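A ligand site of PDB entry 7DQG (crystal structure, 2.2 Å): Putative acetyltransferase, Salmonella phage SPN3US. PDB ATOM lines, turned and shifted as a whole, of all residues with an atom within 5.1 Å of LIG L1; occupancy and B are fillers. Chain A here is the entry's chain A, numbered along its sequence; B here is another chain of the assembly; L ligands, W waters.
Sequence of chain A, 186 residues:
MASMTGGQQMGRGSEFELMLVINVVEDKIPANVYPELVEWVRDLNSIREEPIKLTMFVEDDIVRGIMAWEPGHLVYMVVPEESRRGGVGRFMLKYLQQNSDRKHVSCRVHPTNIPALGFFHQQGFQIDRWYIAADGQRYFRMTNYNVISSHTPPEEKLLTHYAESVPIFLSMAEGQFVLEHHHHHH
The backbone NH (N) of Arg 85 is in hydrogen-bond range of an oxygen (O11) of LIG L1 (2.8 Å). O3 of LIG L1 lies within salt-bridge range of NH2 of Arg 85, 2.6 Å away. N of Gly 89 is in hydrogen-bond range of O12 of LIG L1 (2.8 Å). An oxygen (O15) of LIG L1 lies within hydrogen-bond range of the backbone NH (N) of Val 79, at 2.8 Å. The backbone NH (N) of Gly 87 sits at hydrogen-bond distance from an oxygen (O9) of LIG L1, at 2.8 Å. The backbone carbonyl oxygen (O) of Met 77 is in hydrogen-bond range of a nitrogen (N7) of LIG L1, 2.9 Å away. N of Arg 90 lies within hydrogen-bond range of O8 of LIG L1, 2.9 Å away. An oxygen (O16) of LIG L1 lies within hydrogen-bond range of the side-chain amide nitrogen of Asn 113 (3.1 Å). The backbone NH of Gly 86 lies within hydrogen-bond range of an oxygen (O9) of LIG L1, at 3.1 Å. NE2 of Gln 123 lies close to O6 of LIG L1 (3.5 Å).
The backbone carbonyl oxygen (O) of Val 79 is in hydrogen-bond range of the guanidinium group (NE) of Arg 84 (2.7 Å). The backbone NH (N) of Ala 116 lies within hydrogen-bond range of the side-chain amide oxygen (OD1) of Asn 113 (3.3 Å). The side-chain carboxylate of Glu 156 of chain B lies within hydrogen-bond range of the side-chain hydroxyl of Tyr 76, 2.6 Å away. The side-chain amide nitrogen (NE2) of Gln 123 sits close to the backbone carbonyl oxygen (O) of Phe 119 (3.3 Å).
The backbone carbonyl oxygen (O) of Arg 108 lies close to an oxygen (O17) of LIG L1 (3.0 Å). Merely in contact with LIG L1: Gln 122, Glu 156 of chain B, Arg 84, Phe 119, Pro 115, Val 78, Tyr 76, Leu 74, Val 88, Cys 107, Phe 120, Gly 118 and Ala 116. Hydrophobic or aromatic side chains that line LIG L1: Leu 74, Tyr 76, Met 77, Val 78, Val 79, Val 88, Pro 115, Ala 116, Phe 119 and Phe 120. Within 4 Å of LIG L1: Leu 74, Tyr 76, Met 77, Val 78, Val 79, Arg 84, Arg 85, Gly 86, Gly 87, Val 88, Gly 89, Arg 90, Cys 107, Arg 108, Asn 113, Pro 115, Ala 116, Gly 118, Phe 119, Phe 120, Gln 122, Gln 123 and Glu 156 of chain B.
Water W3 lies within hydrogen-bond range of an oxygen (O4) of LIG L1 and the backbone NH (N) of Gly 87. Water W1 lies within hydrogen-bond range of O16 of LIG L1 (2.7 Å) and OD1 of Asn 113 (2.8 Å). Water W2 bridges NH1 of Arg 90 (2.8 Å) and NE2 of Gln 123 (3.1 Å).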
ATOM      1  N   LEU A  74      -8.911 -29.914  10.914  1.00  0.00           N
ATOM      2  CA  LEU A  74      -8.217 -30.226   9.677  1.00  0.00           C
ATOM      3  C   LEU A  74      -7.143 -31.268   9.962  1.00  0.00           C
ATOM      4  O   LEU A  74      -6.282 -31.047  10.821  1.00  0.00           O
ATOM      5  CB  LEU A  74      -7.601 -28.964   9.071  1.00  0.00           C
ATOM      6  CG  LEU A  74      -6.550 -29.146   7.979  1.00  0.00           C
ATOM      7  CD1 LEU A  74      -7.127 -29.857   6.761  1.00  0.00           C
ATOM      8  CD2 LEU A  74      -5.962 -27.800   7.586  1.00  0.00           C
ATOM      9  N   VAL A  75      -7.196 -32.393   9.254  1.00  0.00           N
ATOM     10  CA  VAL A  75      -6.214 -33.450   9.440  1.00  0.00           C
ATOM     11  C   VAL A  75      -5.009 -33.172   8.548  1.00  0.00           C
ATOM     12  O   VAL A  75      -3.882 -33.035   9.033  1.00  0.00           O
ATOM     13  CB  VAL A  75      -6.816 -34.839   9.153  1.00  0.00           C
ATOM     14  CG1 VAL A  75      -5.739 -35.909   9.282  1.00  0.00           C
ATOM     15  CG2 VAL A  75      -7.968 -35.117  10.091  1.00  0.00           C
ATOM     16  N   TYR A  76      -5.247 -33.078   7.237  1.00  0.00           N
ATOM     17  CA  TYR A  76      -4.185 -32.714   6.308  1.00  0.00           C
ATOM     18  C   TYR A  76      -4.806 -32.181   5.025  1.00  0.00           C
ATOM     19  O   TYR A  76      -5.895 -32.583   4.627  1.00  0.00           O
ATOM     20  CB  TYR A  76      -3.254 -33.884   5.998  1.00  0.00           C
ATOM     21  CG  TYR A  76      -1.838 -33.454   5.679  1.00  0.00           C
ATOM     22  CD1 TYR A  76      -0.909 -33.240   6.692  1.00  0.00           C
ATOM     23  CD2 TYR A  76      -1.431 -33.261   4.364  1.00  0.00           C
ATOM     24  CE1 TYR A  76       0.378 -32.843   6.398  1.00  0.00           C
ATOM     25  CE2 TYR A  76      -0.141 -32.864   4.060  1.00  0.00           C
ATOM     26  CZ  TYR A  76       0.761 -32.655   5.086  1.00  0.00           C
ATOM     27  OH  TYR A  76       2.047 -32.258   4.802  1.00  0.00           O
ATOM     28  N   MET A  77      -4.074 -31.276   4.370  1.00  0.00           N
ATOM     29  CA  MET A  77      -4.447 -30.729   3.075  1.00  0.00           C
ATOM     30  C   MET A  77      -3.183 -30.504   2.271  1.00  0.00           C
ATOM     31  O   MET A  77      -2.114 -30.229   2.826  1.00  0.00           O
ATOM     32  CB  MET A  77      -5.243 -29.421   3.217  1.00  0.00           C
ATOM     33  CG  MET A  77      -4.370 -28.178   3.379  1.00  0.00           C
ATOM     34  SD  MET A  77      -5.278 -26.683   3.806  1.00  0.00           S
ATOM     35  CE  MET A  77      -6.060 -26.279   2.258  1.00  0.00           C
ATOM     36  N   VAL A  78      -3.300 -30.625   0.947  1.00  0.00           N
ATOM     37  CA  VAL A  78      -2.168 -30.349   0.076  1.00  0.00           C
ATOM     38  C   VAL A  78      -2.694 -29.829  -1.263  1.00  0.00           C
ATOM     39  O   VAL A  78      -3.634 -30.392  -1.831  1.00  0.00           O
ATOM     40  CB  VAL A  78      -1.266 -31.585  -0.128  1.00  0.00           C
ATOM     41  CG1 VAL A  78      -2.091 -32.818  -0.432  1.00  0.00           C
ATOM     42  CG2 VAL A  78      -0.234 -31.331  -1.225  1.00  0.00           C
ATOM     43  N   VAL A  79      -2.104 -28.742  -1.735  1.00  0.00           N
ATOM     44  CA  VAL A  79      -2.279 -28.260  -3.102  1.00  0.00           C
ATOM     45  C   VAL A  79      -1.051 -28.693  -3.890  1.00  0.00           C
ATOM     46  O   VAL A  79       0.074 -28.352  -3.484  1.00  0.00           O
ATOM     47  CB  VAL A  79      -2.442 -26.729  -3.140  1.00  0.00           C
ATOM     48  CG1 VAL A  79      -2.486 -26.247  -4.584  1.00  0.00           C
ATOM     49  CG2 VAL A  79      -3.691 -26.307  -2.388  1.00  0.00           C
ATOM     50  N   SER A  83      -0.367 -25.890  -8.687  1.00  0.00           N
ATOM     51  CA  SER A  83      -1.619 -25.179  -8.427  1.00  0.00           C
ATOM     52  C   SER A  83      -1.513 -24.217  -7.252  1.00  0.00           C
ATOM     53  O   SER A  83      -2.539 -23.656  -6.829  1.00  0.00           O
ATOM     54  CB  SER A  83      -2.752 -26.177  -8.198  1.00  0.00           C
ATOM     55  OG  SER A  83      -3.114 -26.830  -9.397  1.00  0.00           O
ATOM     56  N   ARG A  84      -0.319 -23.989  -6.714  1.00  0.00           N
ATOM     57  CA  ARG A  84      -0.177 -23.232  -5.481  1.00  0.00           C
ATOM     58  C   ARG A  84      -0.204 -21.730  -5.752  1.00  0.00           C
ATOM     59  O   ARG A  84      -0.070 -21.265  -6.887  1.00  0.00           O
ATOM     60  CB  ARG A  84       1.118 -23.626  -4.765  1.00  0.00           C
ATOM     61  CG  ARG A  84       0.972 -24.864  -3.903  1.00  0.00           C
ATOM     62  CD  ARG A  84       2.304 -25.386  -3.398  1.00  0.00           C
ATOM     63  NE  ARG A  84       2.217 -26.796  -3.052  1.00  0.00           N
ATOM     64  CZ  ARG A  84       3.257 -27.554  -2.697  1.00  0.00           C
ATOM     65  NH1 ARG A  84       4.471 -27.026  -2.625  1.00  0.00           N
ATOM     66  NH2 ARG A  84       3.073 -28.831  -2.407  1.00  0.00           N
ATOM     67  N   ARG A  85      -0.387 -20.965  -4.673  1.00  0.00           N
ATOM     68  CA  ARG A  85      -0.417 -19.496  -4.707  1.00  0.00           C
ATOM     69  C   ARG A  85      -1.494 -18.989  -5.660  1.00  0.00           C
ATOM     70  O   ARG A  85      -1.325 -17.981  -6.346  1.00  0.00           O
ATOM     71  CB  ARG A  85       0.947 -18.924  -5.079  1.00  0.00           C
ATOM     72  CG  ARG A  85       2.106 -19.420  -4.206  1.00  0.00           C
ATOM     73  CD  ARG A  85       1.818 -19.228  -2.724  1.00  0.00           C
ATOM     74  NE  ARG A  85       1.803 -17.817  -2.329  1.00  0.00           N
ATOM     75  CZ  ARG A  85       2.800 -17.199  -1.702  1.00  0.00           C
ATOM     76  NH1 ARG A  85       3.898 -17.867  -1.390  1.00  0.00           N
ATOM     77  NH2 ARG A  85       2.685 -15.911  -1.390  1.00  0.00           N
ATOM     78  N   GLY A  86      -2.642 -19.674  -5.687  1.00  0.00           N
ATOM     79  CA  GLY A  86      -3.744 -19.269  -6.536  1.00  0.00           C
ATOM     80  C   GLY A  86      -5.053 -19.154  -5.788  1.00  0.00           C
ATOM     81  O   GLY A  86      -6.102 -18.930  -6.387  1.00  0.00           O
ATOM     82  N   GLY A  87      -4.994 -19.297  -4.456  1.00  0.00           N
ATOM     83  CA  GLY A  87      -6.175 -19.233  -3.632  1.00  0.00           C
ATOM     84  C   GLY A  87      -6.878 -20.547  -3.394  1.00  0.00           C
ATOM     85  O   GLY A  87      -7.897 -20.561  -2.703  1.00  0.00           O
ATOM     86  N   VAL A  88      -6.372 -21.651  -3.956  1.00  0.00           N
ATOM     87  CA  VAL A  88      -7.021 -22.946  -3.775  1.00  0.00           C
ATOM     88  C   VAL A  88      -7.020 -23.326  -2.299  1.00  0.00           C
ATOM     89  O   VAL A  88      -8.049 -23.738  -1.746  1.00  0.00           O
ATOM     90  CB  VAL A  88      -6.335 -24.016  -4.628  1.00  0.00           C
ATOM     91  CG1 VAL A  88      -7.074 -25.342  -4.505  1.00  0.00           C
ATOM     92  CG2 VAL A  88      -6.269 -23.579  -6.084  1.00  0.00           C
ATOM     93  N   GLY A  89      -5.864 -23.221  -1.641  1.00  0.00           N
ATOM     94  CA  GLY A  89      -5.793 -23.519  -0.226  1.00  0.00           C
ATOM     95  C   GLY A  89      -6.754 -22.685   0.596  1.00  0.00           C
ATOM     96  O   GLY A  89      -7.409 -23.192   1.522  1.00  0.00           O
ATOM     97  N   ARG A  90      -6.877 -21.400   0.272  1.00  0.00           N
ATOM     98  CA  ARG A  90      -7.823 -20.540   0.974  1.00  0.00           C
ATOM     99  C   ARG A  90      -9.259 -20.998   0.768  1.00  0.00           C
ATOM    100  O   ARG A  90     -10.082 -20.942   1.682  1.00  0.00           O
ATOM    101  CB  ARG A  90      -7.646 -19.090   0.531  1.00  0.00           C
ATOM    102  CG  ARG A  90      -8.589 -18.102   1.216  1.00  0.00           C
ATOM    103  CD  ARG A  90      -8.264 -16.657   0.876  1.00  0.00           C
ATOM    104  NE  ARG A  90      -8.269 -16.428  -0.563  1.00  0.00           N
ATOM    105  CZ  ARG A  90      -7.213 -16.011  -1.265  1.00  0.00           C
ATOM    106  NH1 ARG A  90      -6.053 -15.783  -0.654  1.00  0.00           N
ATOM    107  NH2 ARG A  90      -7.309 -15.815  -2.575  1.00  0.00           N
ATOM    108  N   CYS A 107      -5.832 -27.305  13.763  1.00  0.00           N
ATOM    109  CA  CYS A 107      -4.930 -28.039  12.896  1.00  0.00           C
ATOM    110  C   CYS A 107      -3.603 -28.251  13.615  1.00  0.00           C
ATOM    111  O   CYS A 107      -3.331 -27.660  14.662  1.00  0.00           O
ATOM    112  CB  CYS A 107      -4.749 -27.319  11.552  1.00  0.00           C
ATOM    113  SG  CYS A 107      -3.654 -25.895  11.542  1.00  0.00           S
ATOM    114  N   ARG A 108      -2.787 -29.134  13.053  1.00  0.00           N
ATOM    115  CA  ARG A 108      -1.456 -29.450  13.563  1.00  0.00           C
ATOM    116  C   ARG A 108      -0.434 -29.188  12.474  1.00  0.00           C
ATOM    117  O   ARG A 108      -0.627 -29.582  11.320  1.00  0.00           O
ATOM    118  CB  ARG A 108      -1.365 -30.903  14.019  1.00  0.00           C
ATOM    119  CG  ARG A 108      -2.215 -31.250  15.227  1.00  0.00           C
ATOM    120  CD  ARG A 108      -1.964 -32.681  15.676  1.00  0.00           C
ATOM    121  NE  ARG A 108      -2.686 -32.998  16.910  1.00  0.00           N
ATOM    122  CZ  ARG A 108      -2.792 -34.223  17.421  1.00  0.00           C
ATOM    123  NH1 ARG A 108      -2.222 -35.246  16.817  1.00  0.00           N
ATOM    124  NH2 ARG A 108      -3.470 -34.411  18.546  1.00  0.00           N
ATOM    125  N   VAL A 109       0.663 -28.516  12.840  1.00  0.00           N
ATOM    126  CA  VAL A 109       1.719 -28.172  11.898  1.00  0.00           C
ATOM    127  C   VAL A 109       3.063 -28.419  12.569  1.00  0.00           C
ATOM    128  O   VAL A 109       3.287 -27.991  13.702  1.00  0.00           O
ATOM    129  CB  VAL A 109       1.627 -26.711  11.420  1.00  0.00           C
ATOM    130  CG1 VAL A 109       2.652 -26.449  10.322  1.00  0.00           C
ATOM    131  CG2 VAL A 109       0.224 -26.369  10.943  1.00  0.00           C
ATOM    132  N   ASN A 113       7.649 -26.769   9.199  1.00  0.00           N
ATOM    133  CA  ASN A 113       6.772 -26.393   8.090  1.00  0.00           C
ATOM    134  C   ASN A 113       6.341 -24.925   8.225  1.00  0.00           C
ATOM    135  O   ASN A 113       5.163 -24.598   8.340  1.00  0.00           O
ATOM    136  CB  ASN A 113       5.566 -27.327   8.020  1.00  0.00           C
ATOM    137  CG  ASN A 113       4.868 -27.281   6.673  1.00  0.00           C
ATOM    138  OD1 ASN A 113       5.198 -26.451   5.820  1.00  0.00           O
ATOM    139  ND2 ASN A 113       3.893 -28.158   6.482  1.00  0.00           N
ATOM    140  N   PRO A 115       6.448 -22.530   5.916  1.00  0.00           N
ATOM    141  CA  PRO A 115       5.511 -22.101   4.854  1.00  0.00           C
ATOM    142  C   PRO A 115       4.041 -22.349   5.195  1.00  0.00           C
ATOM    143  O   PRO A 115       3.204 -21.478   4.920  1.00  0.00           O
ATOM    144  CB  PRO A 115       5.957 -22.940   3.649  1.00  0.00           C
ATOM    145  CG  PRO A 115       7.415 -23.124   3.855  1.00  0.00           C
ATOM    146  CD  PRO A 115       7.614 -23.239   5.352  1.00  0.00           C
ATOM    147  N   ALA A 116       3.710 -23.507   5.769  1.00  0.00           N
ATOM    148  CA  ALA A 116       2.322 -23.744   6.164  1.00  0.00           C
ATOM    149  C   ALA A 116       1.896 -22.802   7.284  1.00  0.00           C
ATOM    150  O   ALA A 116       0.745 -22.344   7.295  1.00  0.00           O
ATOM    151  CB  ALA A 116       2.140 -25.199   6.596  1.00  0.00           C
ATOM    152  N   GLY A 118       2.844 -19.761   7.605  1.00  0.00           N
ATOM    153  CA  GLY A 118       2.519 -18.511   6.933  1.00  0.00           C
ATOM    154  C   GLY A 118       1.150 -18.554   6.268  1.00  0.00           C
ATOM    155  O   GLY A 118       0.396 -17.579   6.320  1.00  0.00           O
ATOM    156  N   PHE A 119       0.821 -19.688   5.649  1.00  0.00           N
ATOM    157  CA  PHE A 119      -0.496 -19.823   5.027  1.00  0.00           C
ATOM    158  C   PHE A 119      -1.601 -19.683   6.061  1.00  0.00           C
ATOM    159  O   PHE A 119      -2.499 -18.849   5.914  1.00  0.00           O
ATOM    160  CB  PHE A 119      -0.606 -21.177   4.308  1.00  0.00           C
ATOM    161  CG  PHE A 119      -2.014 -21.566   3.946  1.00  0.00           C
ATOM    162  CD1 PHE A 119      -2.680 -20.914   2.924  1.00  0.00           C
ATOM    163  CD2 PHE A 119      -2.678 -22.565   4.638  1.00  0.00           C
ATOM    164  CE1 PHE A 119      -3.988 -21.256   2.591  1.00  0.00           C
ATOM    165  CE2 PHE A 119      -3.979 -22.915   4.307  1.00  0.00           C
ATOM    166  CZ  PHE A 119      -4.622 -22.258   3.281  1.00  0.00           C
ATOM    167  N   PHE A 120      -1.553 -20.495   7.125  1.00  0.00           N
ATOM    168  CA  PHE A 120      -2.617 -20.471   8.126  1.00  0.00           C
ATOM    169  C   PHE A 120      -2.700 -19.120   8.822  1.00  0.00           C
ATOM    170  O   PHE A 120      -3.790 -18.624   9.111  1.00  0.00           O
ATOM    171  CB  PHE A 120      -2.410 -21.593   9.142  1.00  0.00           C
ATOM    172  CG  PHE A 120      -2.626 -22.974   8.579  1.00  0.00           C
ATOM    173  CD1 PHE A 120      -3.860 -23.343   8.079  1.00  0.00           C
ATOM    174  CD2 PHE A 120      -1.593 -23.890   8.554  1.00  0.00           C
ATOM    175  CE1 PHE A 120      -4.066 -24.606   7.553  1.00  0.00           C
ATOM    176  CE2 PHE A 120      -1.793 -25.160   8.030  1.00  0.00           C
ATOM    177  CZ  PHE A 120      -3.026 -25.515   7.531  1.00  0.00           C
ATOM    178  N   GLN A 122      -2.041 -16.214   7.532  1.00  0.00           N
ATOM    179  CA  GLN A 122      -2.744 -15.309   6.631  1.00  0.00           C
ATOM    180  C   GLN A 122      -4.247 -15.564   6.609  1.00  0.00           C
ATOM    181  O   GLN A 122      -5.003 -14.666   6.213  1.00  0.00           O
ATOM    182  CB  GLN A 122      -2.165 -15.439   5.211  1.00  0.00           C
ATOM    183  CG  GLN A 122      -2.469 -14.257   4.304  1.00  0.00           C
ATOM    184  CD  GLN A 122      -1.806 -12.967   4.761  1.00  0.00           C
ATOM    185  OE1 GLN A 122      -0.818 -12.993   5.494  1.00  0.00           O
ATOM    186  NE2 GLN A 122      -2.351 -11.845   4.325  1.00  0.00           N
ATOM    187  N   GLN A 123      -4.689 -16.753   7.016  1.00  0.00           N
ATOM    188  CA  GLN A 123      -6.110 -17.084   7.067  1.00  0.00           C
ATOM    189  C   GLN A 123      -6.727 -16.813   8.439  1.00  0.00           C
ATOM    190  O   GLN A 123      -7.874 -17.226   8.668  1.00  0.00           O
ATOM    191  CB  GLN A 123      -6.323 -18.545   6.680  1.00  0.00           C
ATOM    192  CG  GLN A 123      -5.541 -18.980   5.454  1.00  0.00           C
ATOM    193  CD  GLN A 123      -5.702 -18.018   4.291  1.00  0.00           C
ATOM    194  OE1 GLN A 123      -6.820 -17.678   3.903  1.00  0.00           O
ATOM    195  NE2 GLN A 123      -4.579 -17.572   3.733  1.00  0.00           N
ATOM    196  N   GLU B 156       1.623 -36.606   2.818  1.00  0.00           N
ATOM    197  CA  GLU B 156       1.651 -35.603   1.760  1.00  0.00           C
ATOM    198  C   GLU B 156       1.917 -36.241   0.406  1.00  0.00           C
ATOM    199  O   GLU B 156       1.298 -35.857  -0.599  1.00  0.00           O
ATOM    200  CB  GLU B 156       2.717 -34.541   2.065  1.00  0.00           C
ATOM    201  CG  GLU B 156       2.778 -33.414   1.041  1.00  0.00           C
ATOM    202  CD  GLU B 156       3.628 -32.248   1.495  1.00  0.00           C
ATOM    203  OE1 GLU B 156       3.589 -31.900   2.698  1.00  0.00           O
ATOM    204  OE2 GLU B 156       4.350 -31.673   0.652  1.00  0.00           O
HETATM  205  N1  LIG L   1       4.691 -19.125   2.539  1.00  0.00           N
HETATM  206  C1  LIG L   1       4.203 -18.037   3.137  1.00  0.00           C
HETATM  207  N2  LIG L   1       2.935 -17.689   2.998  1.00  0.00           N
HETATM  208  C2  LIG L   1       2.095 -18.415   2.246  1.00  0.00           C
HETATM  209  C3  LIG L   1       2.580 -19.550   1.616  1.00  0.00           C
HETATM  210  C4  LIG L   1       3.937 -19.900   1.779  1.00  0.00           C
HETATM  211  N3  LIG L   1       4.480 -21.082   1.133  1.00  0.00           N
HETATM  212  N4  LIG L   1       1.557 -20.085   0.931  1.00  0.00           N
HETATM  213  C5  LIG L   1       0.481 -19.337   1.127  1.00  0.00           C
HETATM  214  N5  LIG L   1       0.792 -18.325   1.925  1.00  0.00           N
HETATM  215  C6  LIG L   1      -0.034 -17.367   2.310  1.00  0.00           C
HETATM  216  C7  LIG L   1       0.118 -16.123   1.325  1.00  0.00           C
HETATM  217  O1  LIG L   1      -0.136 -14.836   2.055  1.00  0.00           O
HETATM  218  C8  LIG L   1      -0.981 -16.410   0.366  1.00  0.00           C
HETATM  219  O2  LIG L   1      -1.458 -15.175  -0.297  1.00  0.00           O
HETATM  220  P1  LIG L   1      -0.636 -14.655  -1.633  1.00  0.00           P
HETATM  221  O3  LIG L   1       0.722 -14.143  -1.230  1.00  0.00           O
HETATM  222  O4  LIG L   1      -0.467 -15.809  -2.591  1.00  0.00           O
HETATM  223  O5  LIG L   1      -1.419 -13.549  -2.302  1.00  0.00           O
HETATM  224  C9  LIG L   1      -2.120 -17.049   1.391  1.00  0.00           C
HETATM  225  O6  LIG L   1      -1.490 -17.808   2.213  1.00  0.00           O
HETATM  226  C10 LIG L   1      -3.135 -17.856   0.599  1.00  0.00           C
HETATM  227  O7  LIG L   1      -2.431 -18.596  -0.355  1.00  0.00           O
HETATM  228  P2  LIG L   1      -3.151 -19.873  -1.108  1.00  0.00           P
HETATM  229  O8  LIG L   1      -4.628 -19.904  -0.816  1.00  0.00           O
HETATM  230  O9  LIG L   1      -2.925 -19.768  -2.600  1.00  0.00           O
HETATM  231  O10 LIG L   1      -2.462 -21.257  -0.545  1.00  0.00           O
HETATM  232  P3  LIG L   1      -2.107 -22.556  -1.486  1.00  0.00           P
HETATM  233  O11 LIG L   1      -0.842 -22.311  -2.258  1.00  0.00           O
HETATM  234  O12 LIG L   1      -3.246 -22.811  -2.445  1.00  0.00           O
HETATM  235  O13 LIG L   1      -1.927 -23.859  -0.492  1.00  0.00           O
HETATM  236  C11 LIG L   1      -0.699 -24.984   1.173  1.00  0.00           C
HETATM  237  C12 LIG L   1      -1.352 -23.669   0.775  1.00  0.00           C
HETATM  238  C13 LIG L   1      -1.797 -26.014   1.422  1.00  0.00           C
HETATM  239  C14 LIG L   1       0.119 -24.781   2.446  1.00  0.00           C
HETATM  240  C15 LIG L   1       0.212 -25.406   0.016  1.00  0.00           C
HETATM  241  O14 LIG L   1       1.307 -24.542  -0.020  1.00  0.00           O
HETATM  242  C16 LIG L   1       0.731 -26.844   0.135  1.00  0.00           C
HETATM  243  O15 LIG L   1       0.111 -27.739  -0.331  1.00  0.00           O
HETATM  244  N6  LIG L   1       1.997 -27.091   0.795  1.00  0.00           N
HETATM  245  C17 LIG L   1       2.538 -28.432   0.923  1.00  0.00           C
HETATM  246  C18 LIG L   1       1.644 -29.320   1.793  1.00  0.00           C
HETATM  247  C19 LIG L   1       1.453 -28.755   3.197  1.00  0.00           C
HETATM  248  O16 LIG L   1       2.390 -28.344   3.802  1.00  0.00           O
HETATM  249  N7  LIG L   1       0.135 -28.731   3.785  1.00  0.00           N
HETATM  250  C20 LIG L   1      -0.030 -28.208   5.133  1.00  0.00           C
HETATM  251  C21 LIG L   1       0.298 -29.331   6.111  1.00  0.00           C
HETATM  252  S1  LIG L   1      -0.241 -28.949   7.798  1.00  0.00           S
HETATM  253  C22 LIG L   1      -2.040 -29.172   7.953  1.00  0.00           C
HETATM  254  O17 LIG L   1      -2.562 -29.093   9.014  1.00  0.00           O
HETATM  255  C23 LIG L   1      -2.871 -29.469   6.716  1.00  0.00           C
HETATM  256  N1  LG2 L   2       6.277 -13.501   4.933  1.00  0.00           N
HETATM  257  C1  LG2 L   2       6.772 -14.638   4.451  1.00  0.00           C
HETATM  258  N2  LG2 L   2       7.988 -14.692   3.928  1.00  0.00           N
HETATM  259  C2  LG2 L   2       8.761 -13.599   3.860  1.00  0.00           C
HETATM  260  C3  LG2 L   2       8.268 -12.407   4.355  1.00  0.00           C
HETATM  261  C4  LG2 L   2       6.969 -12.375   4.906  1.00  0.00           C
HETATM  262  N3  LG2 L   2       6.412 -11.136   5.435  1.00  0.00           N
HETATM  263  N4  LG2 L   2       9.218 -11.481   4.176  1.00  0.00           N
HETATM  264  C5  LG2 L   2      10.261 -12.057   3.602  1.00  0.00           C
HETATM  265  N5  LG2 L   2       9.999 -13.339   3.403  1.00  0.00           N
HETATM  266  C6  LG2 L   2      10.816 -14.222   2.840  1.00  0.00           C
HETATM  267  C7  LG2 L   2      10.453 -14.325   1.292  1.00  0.00           C
HETATM  268  O1  LG2 L   2      10.724 -15.710   0.783  1.00  0.00           O
HETATM  269  C8  LG2 L   2      11.428 -13.353   0.717  1.00  0.00           C
HETATM  270  O2  LG2 L   2      11.735 -13.658  -0.690  1.00  0.00           O
HETATM  271  P1  LG2 L   2      10.715 -13.068  -1.843  1.00  0.00           P
HETATM  272  O3  LG2 L   2       9.391 -13.784  -1.775  1.00  0.00           O
HETATM  273  O4  LG2 L   2      10.481 -11.588  -1.591  1.00  0.00           O
HETATM  274  O5  LG2 L   2      11.333 -13.260  -3.213  1.00  0.00           O
HETATM  275  C9  LG2 L   2      12.730 -13.620   1.719  1.00  0.00           C
HETATM  276  O6  LG2 L   2      12.268 -13.766   2.905  1.00  0.00           O
HETATM  277  C10 LG2 L   2      13.680 -12.437   1.662  1.00  0.00           C
HETATM  278  O7  LG2 L   2      12.896 -11.272   1.680  1.00  0.00           O
HETATM  279  P2  LG2 L   2      13.583  -9.816   2.033  1.00  0.00           P
HETATM  280  O8  LG2 L   2      15.094  -9.931   2.048  1.00  0.00           O
HETATM  281  O9  LG2 L   2      13.156  -8.795   1.005  1.00  0.00           O
HETATM  282  O10 LG2 L   2      13.061  -9.355   3.530  1.00  0.00           O
HETATM  283  P3  LG2 L   2      12.662  -7.810   3.924  1.00  0.00           P
HETATM  284  O11 LG2 L   2      11.292  -7.477   3.404  1.00  0.00           O
HETATM  285  O12 LG2 L   2      13.680  -6.862   3.319  1.00  0.00           O
HETATM  286  O13 LG2 L   2      12.698  -7.690   5.568  1.00  0.00           O
HETATM  287  C11 LG2 L   2      11.780  -8.253   7.655  1.00  0.00           C
HETATM  288  C12 LG2 L   2      12.291  -8.794   6.330  1.00  0.00           C
HETATM  289  C13 LG2 L   2      12.955  -7.680   8.445  1.00  0.00           C
HETATM  290  C14 LG2 L   2      11.126  -9.379   8.451  1.00  0.00           C
HETATM  291  C15 LG2 L   2      10.742  -7.163   7.340  1.00  0.00           C
HETATM  292  O14 LG2 L   2       9.605  -7.782   6.819  1.00  0.00           O
HETATM  293  C16 LG2 L   2      10.339  -6.328   8.547  1.00  0.00           C
HETATM  294  O15 LG2 L   2      10.939  -5.344   8.823  1.00  0.00           O
HETATM  295  N6  LG2 L   2       9.186  -6.726   9.336  1.00  0.00           N
HETATM  296  C17 LG2 L   2       8.747  -5.956  10.489  1.00  0.00           C
HETATM  297  C18 LG2 L   2       9.805  -5.957  11.596  1.00  0.00           C
HETATM  298  C19 LG2 L   2      10.147  -7.362  12.071  1.00  0.00           C
HETATM  299  O16 LG2 L   2       9.280  -8.149  12.297  1.00  0.00           O
HETATM  300  N7  LG2 L   2      11.536  -7.745  12.264  1.00  0.00           N
HETATM  301  C20 LG2 L   2      11.850  -9.084  12.733  1.00  0.00           C
HETATM  302  C21 LG2 L   2      11.714  -9.071  14.264  1.00  0.00           C
HETATM  303  S1  LG2 L   2      12.458 -10.554  15.016  1.00  0.00           S
HETATM  304  C22 LG2 L   2      14.267 -10.405  15.038  1.00  0.00           C
HETATM  305  O17 LG2 L   2      14.924 -11.217  15.607  1.00  0.00           O
HETATM  306  C23 LG2 L   2      14.947  -9.242  14.323  1.00  0.00           C
HETATM  307  O   HOH W   1       4.244 -26.410   3.186  1.00  0.00           O
HETATM  308  O   HOH W   2      -5.035 -15.176   1.859  1.00  0.00           O
HETATM  309  O   HOH W   3      -2.769 -17.067  -3.164  1.00  0.00           O
HETATM  310  O   HOH W   4       1.820 -22.199  -1.022  1.00  0.00           O
HETATM  311  O   HOH W   5      -3.599 -22.062  -4.831  1.00  0.00           O
